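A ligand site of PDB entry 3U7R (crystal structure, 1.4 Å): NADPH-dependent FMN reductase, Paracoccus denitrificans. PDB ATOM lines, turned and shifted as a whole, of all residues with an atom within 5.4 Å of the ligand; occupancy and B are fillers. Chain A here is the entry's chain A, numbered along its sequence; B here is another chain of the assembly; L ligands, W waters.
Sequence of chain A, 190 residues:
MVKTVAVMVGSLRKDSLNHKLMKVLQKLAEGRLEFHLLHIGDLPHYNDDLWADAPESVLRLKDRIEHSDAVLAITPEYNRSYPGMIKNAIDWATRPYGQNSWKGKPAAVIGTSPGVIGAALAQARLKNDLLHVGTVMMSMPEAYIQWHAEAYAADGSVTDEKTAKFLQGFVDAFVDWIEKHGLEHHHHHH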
ATOM      1  N   SER A  11      13.552   0.715 -20.415  1.00  0.00           N
ATOM      2  CA  SER A  11      13.408   0.537 -21.844  1.00  0.00           C
ATOM      3  C   SER A  11      14.486   1.346 -22.538  1.00  0.00           C
ATOM      4  O   SER A  11      14.868   2.391 -22.051  1.00  0.00           O
ATOM      5  CB  SER A  11      12.050   1.000 -22.295  1.00  0.00           C
ATOM      6  OG  SER A  11      11.925   0.797 -23.696  1.00  0.00           O
ATOM      7  N   ARG A  13      14.238   1.631 -26.141  1.00  0.00           N
ATOM      8  CA  ARG A  13      13.802   1.900 -27.505  1.00  0.00           C
ATOM      9  C   ARG A  13      13.536   3.393 -27.718  1.00  0.00           C
ATOM     10  O   ARG A  13      13.224   4.125 -26.782  1.00  0.00           O
ATOM     11  CB  ARG A  13      12.549   1.064 -27.853  1.00  0.00           C
ATOM     12  CG  ARG A  13      11.275   1.551 -27.209  1.00  0.00           C
ATOM     13  CD  ARG A  13      10.087   0.668 -27.652  1.00  0.00           C
ATOM     14  NE  ARG A  13       8.815   1.171 -27.090  1.00  0.00           N
ATOM     15  CZ  ARG A  13       7.951   1.905 -27.768  1.00  0.00           C
ATOM     16  NH1 ARG A  13       8.144   2.202 -29.052  1.00  0.00           N
ATOM     17  NH2 ARG A  13       6.842   2.312 -27.167  1.00  0.00           N
ATOM     18  N   ASP A  15      11.104   5.253 -28.939  1.00  0.00           N
ATOM     19  CA  ASP A  15       9.891   5.996 -28.615  1.00  0.00           C
ATOM     20  C   ASP A  15       9.305   5.504 -27.286  1.00  0.00           C
ATOM     21  O   ASP A  15       8.111   5.574 -27.072  1.00  0.00           O
ATOM     22  CB  ASP A  15       8.900   5.922 -29.778  1.00  0.00           C
ATOM     23  CG  ASP A  15       9.345   6.755 -31.018  1.00  0.00           C
ATOM     24  OD1 ASP A  15       9.828   7.907 -30.853  1.00  0.00           O
ATOM     25  OD2 ASP A  15       9.170   6.248 -32.148  1.00  0.00           O
ATOM     26  N   SER A  16      10.142   4.994 -26.405  1.00  0.00           N
ATOM     27  CA  SER A  16       9.698   4.445 -25.122  1.00  0.00           C
ATOM     28  C   SER A  16       8.762   5.342 -24.350  1.00  0.00           C
ATOM     29  O   SER A  16       9.026   6.522 -24.112  1.00  0.00           O
ATOM     30  CB  SER A  16      10.916   4.199 -24.232  1.00  0.00           C
ATOM     31  OG  SER A  16      10.572   3.991 -22.873  1.00  0.00           O
ATOM     32  N   LEU A  17       7.635   4.774 -23.932  1.00  0.00           N
ATOM     33  CA  LEU A  17       6.677   5.481 -23.109  1.00  0.00           C
ATOM     34  C   LEU A  17       7.221   5.680 -21.712  1.00  0.00           C
ATOM     35  O   LEU A  17       6.984   6.716 -21.079  1.00  0.00           O
ATOM     36  CB  LEU A  17       5.360   4.686 -23.037  1.00  0.00           C
ATOM     37  CG  LEU A  17       4.701   4.389 -24.378  1.00  0.00           C
ATOM     38  CD1 LEU A  17       3.383   3.642 -24.173  1.00  0.00           C
ATOM     39  CD2 LEU A  17       4.525   5.676 -25.169  1.00  0.00           C
ATOM     40  N   ASN A  18       7.950   4.701 -21.178  1.00  0.00           N
ATOM     41  CA  ASN A  18       8.581   4.888 -19.884  1.00  0.00           C
ATOM     42  C   ASN A  18       9.658   5.983 -19.867  1.00  0.00           C
ATOM     43  O   ASN A  18       9.780   6.714 -18.873  1.00  0.00           O
ATOM     44  CB  ASN A  18       9.063   3.557 -19.333  1.00  0.00           C
ATOM     45  CG  ASN A  18       7.886   2.696 -18.864  1.00  0.00           C
ATOM     46  OD1 ASN A  18       7.381   2.852 -17.758  1.00  0.00           O
ATOM     47  ND2 ASN A  18       7.364   1.885 -19.756  1.00  0.00           N
ATOM     48  N   HIS A  19      10.350   6.149 -20.989  1.00  0.00           N
ATOM     49  CA  HIS A  19      11.221   7.308 -21.110  1.00  0.00           C
ATOM     50  C   HIS A  19      10.434   8.613 -21.129  1.00  0.00           C
ATOM     51  O   HIS A  19      10.826   9.591 -20.473  1.00  0.00           O
ATOM     52  CB  HIS A  19      12.061   7.209 -22.380  1.00  0.00           C
ATOM     53  CG  HIS A  19      12.946   8.389 -22.613  1.00  0.00           C
ATOM     54  ND1 HIS A  19      12.678   9.347 -23.558  1.00  0.00           N
ATOM     55  CD2 HIS A  19      14.047   8.797 -21.962  1.00  0.00           C
ATOM     56  CE1 HIS A  19      13.631  10.277 -23.529  1.00  0.00           C
ATOM     57  NE2 HIS A  19      14.449   9.979 -22.543  1.00  0.00           N
ATOM     58  N   PRO A  76       8.541  -0.711 -17.692  1.00  0.00           N
ATOM     59  CA  PRO A  76       7.488  -1.397 -18.439  1.00  0.00           C
ATOM     60  C   PRO A  76       7.246  -2.778 -17.851  1.00  0.00           C
ATOM     61  O   PRO A  76       7.957  -3.220 -16.949  1.00  0.00           O
ATOM     62  CB  PRO A  76       8.045  -1.534 -19.825  1.00  0.00           C
ATOM     63  CG  PRO A  76       9.495  -1.557 -19.665  1.00  0.00           C
ATOM     64  CD  PRO A  76       9.835  -0.840 -18.354  1.00  0.00           C
ATOM     65  N   GLU A  77       6.179  -3.377 -18.347  1.00  0.00           N
ATOM     66  CA  GLU A  77       5.857  -4.774 -18.028  1.00  0.00           C
ATOM     67  C   GLU A  77       6.055  -5.641 -19.246  1.00  0.00           C
ATOM     68  O   GLU A  77       5.451  -5.387 -20.315  1.00  0.00           O
ATOM     69  CB  GLU A  77       4.421  -4.834 -17.515  1.00  0.00           C
ATOM     70  CG  GLU A  77       3.923  -6.222 -17.082  1.00  0.00           C
ATOM     71  CD  GLU A  77       2.593  -6.118 -16.421  1.00  0.00           C
ATOM     72  OE1 GLU A  77       2.524  -5.610 -15.296  1.00  0.00           O
ATOM     73  OE2 GLU A  77       1.587  -6.426 -17.120  1.00  0.00           O
ATOM     74  N   TYR A  78       6.879  -6.682 -19.077  1.00  0.00           N
ATOM     75  CA  TYR A  78       7.113  -7.698 -20.093  1.00  0.00           C
ATOM     76  C   TYR A  78       6.681  -9.041 -19.518  1.00  0.00           C
ATOM     77  O   TYR A  78       7.273  -9.525 -18.531  1.00  0.00           O
ATOM     78  CB  TYR A  78       8.565  -7.789 -20.502  1.00  0.00           C
ATOM     79  CG  TYR A  78       9.186  -6.639 -21.279  1.00  0.00           C
ATOM     80  CD1 TYR A  78       8.451  -5.588 -21.842  1.00  0.00           C
ATOM     81  CD2 TYR A  78      10.557  -6.640 -21.464  1.00  0.00           C
ATOM     82  CE1 TYR A  78       9.046  -4.607 -22.579  1.00  0.00           C
ATOM     83  CE2 TYR A  78      11.158  -5.673 -22.183  1.00  0.00           C
ATOM     84  CZ  TYR A  78      10.418  -4.653 -22.716  1.00  0.00           C
ATOM     85  OH  TYR A  78      11.096  -3.672 -23.440  1.00  0.00           O
ATOM     86  N   ASN A  79       5.678  -9.658 -20.115  1.00  0.00           N
ATOM     87  CA  ASN A  79       5.216 -10.971 -19.681  1.00  0.00           C
ATOM     88  C   ASN A  79       4.956 -11.034 -18.189  1.00  0.00           C
ATOM     89  O   ASN A  79       5.327 -11.966 -17.483  1.00  0.00           O
ATOM     90  CB  ASN A  79       6.216 -12.040 -20.139  1.00  0.00           C
ATOM     91  CG  ASN A  79       6.343 -12.048 -21.661  1.00  0.00           C
ATOM     92  OD1 ASN A  79       7.455 -11.788 -22.248  1.00  0.00           O
ATOM     93  ND2 ASN A  79       5.260 -12.304 -22.322  1.00  0.00           N
ATOM     94  N   ARG A  80       4.276  -9.989 -17.712  1.00  0.00           N
ATOM     95  CA  ARG A  80       3.764  -9.920 -16.341  1.00  0.00           C
ATOM     96  C   ARG A  80       4.822  -9.782 -15.251  1.00  0.00           C
ATOM     97  O   ARG A  80       4.498  -9.944 -14.080  1.00  0.00           O
ATOM     98  CB  ARG A  80       2.741 -11.015 -16.034  1.00  0.00           C
ATOM     99  CG  ARG A  80       1.629 -11.125 -17.083  1.00  0.00           C
ATOM    100  CD  ARG A  80       0.877  -9.837 -17.264  1.00  0.00           C
ATOM    101  NE  ARG A  80      -0.175  -9.968 -18.256  1.00  0.00           N
ATOM    102  CZ  ARG A  80      -0.846  -8.944 -18.775  1.00  0.00           C
ATOM    103  NH1 ARG A  80      -0.624  -7.728 -18.346  1.00  0.00           N
ATOM    104  NH2 ARG A  80      -1.762  -9.193 -19.719  1.00  0.00           N
ATOM    105  N   SER A  81       6.046  -9.408 -15.655  1.00  0.00           N
ATOM    106  CA  SER A  81       7.022  -8.886 -14.698  1.00  0.00           C
ATOM    107  C   SER A  81       7.835  -7.797 -15.335  1.00  0.00           C
ATOM    108  O   SER A  81       7.424  -7.301 -16.379  1.00  0.00           O
ATOM    109  CB  SER A  81       7.849 -10.037 -14.128  1.00  0.00           C
ATOM    110  OG  SER A  81       8.630  -9.585 -13.042  1.00  0.00           O
ATOM    111  N   THR A 112       4.579   2.489 -16.835  1.00  0.00           N
ATOM    112  CA  THR A 112       3.434   2.675 -17.710  1.00  0.00           C
ATOM    113  C   THR A 112       3.402   1.604 -18.786  1.00  0.00           C
ATOM    114  O   THR A 112       4.431   1.032 -19.195  1.00  0.00           O
ATOM    115  CB  THR A 112       3.444   4.089 -18.340  1.00  0.00           C
ATOM    116  OG1 THR A 112       2.200   4.339 -19.017  1.00  0.00           O
ATOM    117  CG2 THR A 112       4.573   4.295 -19.283  1.00  0.00           C
ATOM    118  N   SER A 113       2.171   1.310 -19.185  1.00  0.00           N
ATOM    119  CA  SER A 113       1.833   0.458 -20.296  1.00  0.00           C
ATOM    120  C   SER A 113       0.747   1.112 -21.114  1.00  0.00           C
ATOM    121  O   SER A 113      -0.056   1.859 -20.560  1.00  0.00           O
ATOM    122  CB  SER A 113       1.298  -0.877 -19.737  1.00  0.00           C
ATOM    123  OG  SER A 113       0.858  -1.699 -20.784  1.00  0.00           O
ATOM    124  N   PRO A 114       0.663   0.794 -22.403  1.00  0.00           N
ATOM    125  CA  PRO A 114      -0.526   1.229 -23.159  1.00  0.00           C
ATOM    126  C   PRO A 114      -1.804   0.552 -22.651  1.00  0.00           C
ATOM    127  O   PRO A 114      -2.900   1.053 -22.902  1.00  0.00           O
ATOM    128  CB  PRO A 114      -0.188   0.822 -24.609  1.00  0.00           C
ATOM    129  CG  PRO A 114       0.961  -0.094 -24.534  1.00  0.00           C
ATOM    130  CD  PRO A 114       1.649   0.087 -23.242  1.00  0.00           C
ATOM    131  N   GLY A 115      -1.662  -0.602 -22.020  1.00  0.00           N
ATOM    132  CA  GLY A 115      -2.837  -1.353 -21.530  1.00  0.00           C
ATOM    133  C   GLY A 115      -3.315  -0.850 -20.169  1.00  0.00           C
ATOM    134  O   GLY A 115      -2.571  -0.159 -19.437  1.00  0.00           O
ATOM    135  N   ALA A 119       1.276  -1.602 -16.049  1.00  0.00           N
ATOM    136  CA  ALA A 119       2.504  -2.233 -15.580  1.00  0.00           C
ATOM    137  C   ALA A 119       2.476  -2.637 -14.094  1.00  0.00           C
ATOM    138  O   ALA A 119       3.522  -2.800 -13.481  1.00  0.00           O
ATOM    139  CB  ALA A 119       3.740  -1.438 -15.962  1.00  0.00           C
ATOM    140  N   TYR B  46      17.034  -6.686 -24.214  1.00  0.00           N
ATOM    141  CA  TYR B  46      15.804  -6.555 -25.002  1.00  0.00           C
ATOM    142  C   TYR B  46      15.615  -5.102 -25.474  1.00  0.00           C
ATOM    143  O   TYR B  46      15.751  -4.173 -24.688  1.00  0.00           O
ATOM    144  CB  TYR B  46      14.497  -6.980 -24.255  1.00  0.00           C
ATOM    145  CG  TYR B  46      13.361  -7.127 -25.237  1.00  0.00           C
ATOM    146  CD1 TYR B  46      13.093  -8.344 -25.864  1.00  0.00           C
ATOM    147  CD2 TYR B  46      12.616  -6.031 -25.602  1.00  0.00           C
ATOM    148  CE1 TYR B  46      12.106  -8.451 -26.795  1.00  0.00           C
ATOM    149  CE2 TYR B  46      11.666  -6.121 -26.579  1.00  0.00           C
ATOM    150  CZ  TYR B  46      11.430  -7.336 -27.186  1.00  0.00           C
ATOM    151  OH  TYR B  46      10.480  -7.403 -28.215  1.00  0.00           O
ATOM    152  N   ASP B  48      12.918  -3.431 -28.435  1.00  0.00           N
ATOM    153  CA  ASP B  48      11.939  -3.748 -29.452  1.00  0.00           C
ATOM    154  C   ASP B  48      12.323  -3.192 -30.826  1.00  0.00           C
ATOM    155  O   ASP B  48      11.896  -3.733 -31.831  1.00  0.00           O
ATOM    156  CB  ASP B  48      10.532  -3.234 -29.059  1.00  0.00           C
ATOM    157  CG  ASP B  48       9.410  -4.134 -29.528  1.00  0.00           C
ATOM    158  OD1 ASP B  48       9.508  -5.383 -29.477  1.00  0.00           O
ATOM    159  OD2 ASP B  48       8.336  -3.624 -29.915  1.00  0.00           O
ATOM    160  N   ASP B  91      11.852 -13.069 -22.413  1.00  0.00           N
ATOM    161  CA  ASP B  91      11.122 -11.999 -23.100  1.00  0.00           C
ATOM    162  C   ASP B  91      11.444 -11.999 -24.605  1.00  0.00           C
ATOM    163  O   ASP B  91      10.549 -11.931 -25.415  1.00  0.00           O
ATOM    164  CB  ASP B  91      11.399 -10.649 -22.452  1.00  0.00           C
ATOM    165  CG  ASP B  91      10.773 -10.537 -21.086  1.00  0.00           C
ATOM    166  OD1 ASP B  91       9.793 -11.254 -20.766  1.00  0.00           O
ATOM    167  OD2 ASP B  91      11.245  -9.754 -20.240  1.00  0.00           O
ATOM    168  N   THR B  94       9.407 -14.648 -26.475  1.00  0.00           N
ATOM    169  CA  THR B  94       7.960 -14.435 -26.604  1.00  0.00           C
ATOM    170  C   THR B  94       7.589 -13.552 -27.756  1.00  0.00           C
ATOM    171  O   THR B  94       6.413 -13.481 -28.073  1.00  0.00           O
ATOM    172  CB  THR B  94       7.330 -13.802 -25.336  1.00  0.00           C
ATOM    173  OG1 THR B  94       7.861 -12.470 -25.110  1.00  0.00           O
ATOM    174  CG2 THR B  94       7.512 -14.650 -24.121  1.00  0.00           C
ATOM    175  N   ARG B  95       8.535 -12.903 -28.386  1.00  0.00           N
ATOM    176  CA  ARG B  95       8.291 -11.923 -29.433  1.00  0.00           C
ATOM    177  C   ARG B  95       8.775 -12.394 -30.806  1.00  0.00           C
ATOM    178  O   ARG B  95       9.523 -13.356 -30.903  1.00  0.00           O
ATOM    179  CB  ARG B  95       8.911 -10.569 -29.060  1.00  0.00           C
ATOM    180  CG  ARG B  95       8.566 -10.120 -27.651  1.00  0.00           C
ATOM    181  CD  ARG B  95       7.084 -10.042 -27.337  1.00  0.00           C
ATOM    182  NE  ARG B  95       6.520  -8.834 -27.923  1.00  0.00           N
ATOM    183  CZ  ARG B  95       5.370  -8.287 -27.546  1.00  0.00           C
ATOM    184  NH1 ARG B  95       4.985  -7.163 -28.118  1.00  0.00           N
ATOM    185  NH2 ARG B  95       4.621  -8.845 -26.575  1.00  0.00           N
HETATM  186  C1  LIG L   1       5.162  -6.201 -23.702  1.00  0.00           C
HETATM  187  N1  LIG L   1       4.074  -5.425 -23.323  1.00  0.00           N
HETATM  188  C2  LIG L   1       3.330  -5.794 -22.244  1.00  0.00           C
HETATM  189  N2  LIG L   1       2.419  -4.972 -21.783  1.00  0.00           N
HETATM  190  C3  LIG L   1       1.751  -5.298 -20.714  1.00  0.00           C
HETATM  191  O1  LIG L   1       0.948  -4.468 -20.283  1.00  0.00           O
HETATM  192  N3  LIG L   1       1.926  -6.407 -20.018  1.00  0.00           N
HETATM  193  C4  LIG L   1       2.789  -7.353 -20.419  1.00  0.00           C
HETATM  194  O2  LIG L   1       2.939  -8.431 -19.831  1.00  0.00           O
HETATM  195  C5  LIG L   1       3.599  -7.053 -21.598  1.00  0.00           C
HETATM  196  N4  LIG L   1       4.515  -7.918 -22.054  1.00  0.00           N
HETATM  197  C6  LIG L   1       5.358  -7.503 -23.029  1.00  0.00           C
HETATM  198  C7  LIG L   1       6.405  -8.305 -23.385  1.00  0.00           C
HETATM  199  C8  LIG L   1       7.251  -7.903 -24.360  1.00  0.00           C
HETATM  200  C9  LIG L   1       8.389  -8.850 -24.679  1.00  0.00           C
HETATM  201  C10 LIG L   1       7.047  -6.648 -25.072  1.00  0.00           C
HETATM  202  C11 LIG L   1       7.955  -6.248 -26.206  1.00  0.00           C
HETATM  203  C12 LIG L   1       5.998  -5.838 -24.745  1.00  0.00           C
HETATM  204  C13 LIG L   1       3.787  -4.149 -23.967  1.00  0.00           C
HETATM  205  C14 LIG L   1       4.469  -3.004 -23.355  1.00  0.00           C
HETATM  206  O3  LIG L   1       3.597  -2.585 -22.335  1.00  0.00           O
HETATM  207  C15 LIG L   1       4.595  -1.887 -24.385  1.00  0.00           C
HETATM  208  O4  LIG L   1       5.348  -2.343 -25.512  1.00  0.00           O
HETATM  209  C16 LIG L   1       5.263  -0.718 -23.690  1.00  0.00           C
HETATM  210  O5  LIG L   1       5.052   0.450 -24.511  1.00  0.00           O
HETATM  211  C17 LIG L   1       6.767  -0.924 -23.528  1.00  0.00           C
HETATM  212  O6  LIG L   1       7.320   0.124 -22.724  1.00  0.00           O
HETATM  213  P1  LIG L   1       8.223   1.261 -23.460  1.00  0.00           P
HETATM  214  O7  LIG L   1       8.738   2.109 -22.341  1.00  0.00           O
HETATM  215  O8  LIG L   1       9.306   0.602 -24.270  1.00  0.00           O
HETATM  216  O9  LIG L   1       7.246   1.976 -24.367  1.00  0.00           O
HETATM  217  O   HOH W   1      -1.646  -5.641 -19.998  1.00  0.00           O
HETATM  218  O   HOH W   2       4.613  -1.716 -19.962  1.00  0.00           O
HETATM  219  O   HOH W   3       0.398  -3.904 -17.507  1.00  0.00           O
HETATM  220  O   HOH W   4       9.719  -1.940 -24.922  1.00  0.00           O
HETATM  221  O   HOH W   5       3.855   0.575 -27.053  1.00  0.00           O
HETATM  222  O   HOH W   6       0.759  -7.680 -23.314  1.00  0.00           O
HETATM  223  O   HOH W   7       3.989  -3.208 -27.621  1.00  0.00           O
HETATM  224  O   HOH W   8       7.837  -2.388 -26.729  1.00  0.00           O
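O of Glu 77 sits close to N4 of the ligand. An oxygen (O2) of the ligand sits at hydrogen-bond distance from the backbone NH (N) of Asn 79 (3.0 Å). O7 of the ligand sits at hydrogen-bond distance from OG of Ser 16 (2.7 Å). The backbone NH (N) of Leu 17 is in hydrogen-bond range of an oxygen (O9) of the ligand. The guanidinium group of Arg 13 lies within salt-bridge range of an oxygen (O9) of the ligand (2.8 Å). The side-chain carboxylate (OE2) of Glu 77 is in hydrogen-bond range of a nitrogen (N3) of the ligand (2.9 Å). OG of Ser 113 lies within hydrogen-bond range of O1 of the ligand (2.8 Å). ND2 of Asn 18 is in hydrogen-bond range of O7 of the ligand (2.9 Å). The backbone NH (N) of Asn 18 sits at hydrogen-bond distance from an oxygen (O7) of the ligand, 2.9 Å away. The backbone NH (N) of Arg 80 sits at hydrogen-bond distance from an oxygen (O2) of the ligand (3.0 Å). OG of Ser 11 is in hydrogen-bond range of O8 of the ligand, 2.7 Å away.
OD1 of Asn 79 sits close to OD1 of Asp 91 of chain B (2.8 Å). The backbone NH (N) of Arg 13 is in hydrogen-bond range of the side-chain hydroxyl (OG) of Ser 11, 3.5 Å away. The side-chain hydroxyl (OG1) of Thr 94 of chain B lies within hydrogen-bond range of the side-chain amide oxygen (OD1) of Asn 79 (3.0 Å). OG of Ser 113 lies within hydrogen-bond range of N of Gly 115 (3.0 Å). The side-chain hydroxyl (OH) of Tyr 46 of chain B is in hydrogen-bond range of the side-chain carboxylate (OD1) of Asp 48 of chain B, 2.6 Å away. The side-chain hydroxyl (OG) of Ser 16 sits at hydrogen-bond distance from the backbone NH (N) of Asn 18, at 3.2 Å. O of Asp 91 of chain B sits at hydrogen-bond distance from OG1 of Thr 94 of chain B, at 2.8 Å. The backbone NH (N) of Thr 112 is in hydrogen-bond range of the side-chain amide oxygen (OD1) of Asn 18, 3.0 Å away.
Merely in contact with the ligand: Arg 95 of chain B (3.2 Å), Tyr 78 (3.3 Å), Pro 76 (3.4 Å), Tyr 46 of chain B (3.4 Å), Pro 114 (3.4 Å), Thr 94 of chain B (3.7 Å), Asp 48 of chain B (3.7 Å) and Asp 91 of chain B (3.8 Å). Hydrophobic or aromatic side chains within 4 Å of the ligand: Leu 17, Pro 76, Tyr 78, Pro 114 and Tyr 46 of chain B. Within 4 Å of the ligand: Ser 11, Arg 13, Ser 16, Leu 17, Asn 18, Pro 76, Glu 77, Tyr 78, Asn 79, Arg 80, Ser 113, Pro 114, Tyr 46 of chain B, Asp 48 of chain B, Asp 91 of chain B, Thr 94 of chain B and Arg 95 of chain B.
Water W4 lies within hydrogen-bond range of O8 of the ligand and OH of Tyr 78. Water W2 lies within hydrogen-bond range of an oxygen (O3) of the ligand (2.7 Å), the backbone NH of Glu 77 (2.8 Å) and the backbone carbonyl oxygen of Thr 112 (2.9 Å). Water W8 lies within hydrogen-bond range of an oxygen (O4) of the ligand (2.8 Å) and the side-chain carboxylate of Asp 48 of chain B (3.5 Å). Water W5 lies within hydrogen-bond range of O5 of the ligand and NH2 of Arg 13. Water W1 lies within hydrogen-bond range of the guanidinium group (NH1) of Arg 80 and an oxygen (O1) of the ligand. Water W3 lies within hydrogen-bond range of OE2 of Glu 77 (2.8 Å), N of Ala 119 (2.9 Å) and O1 of the ligand (2.9 Å).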
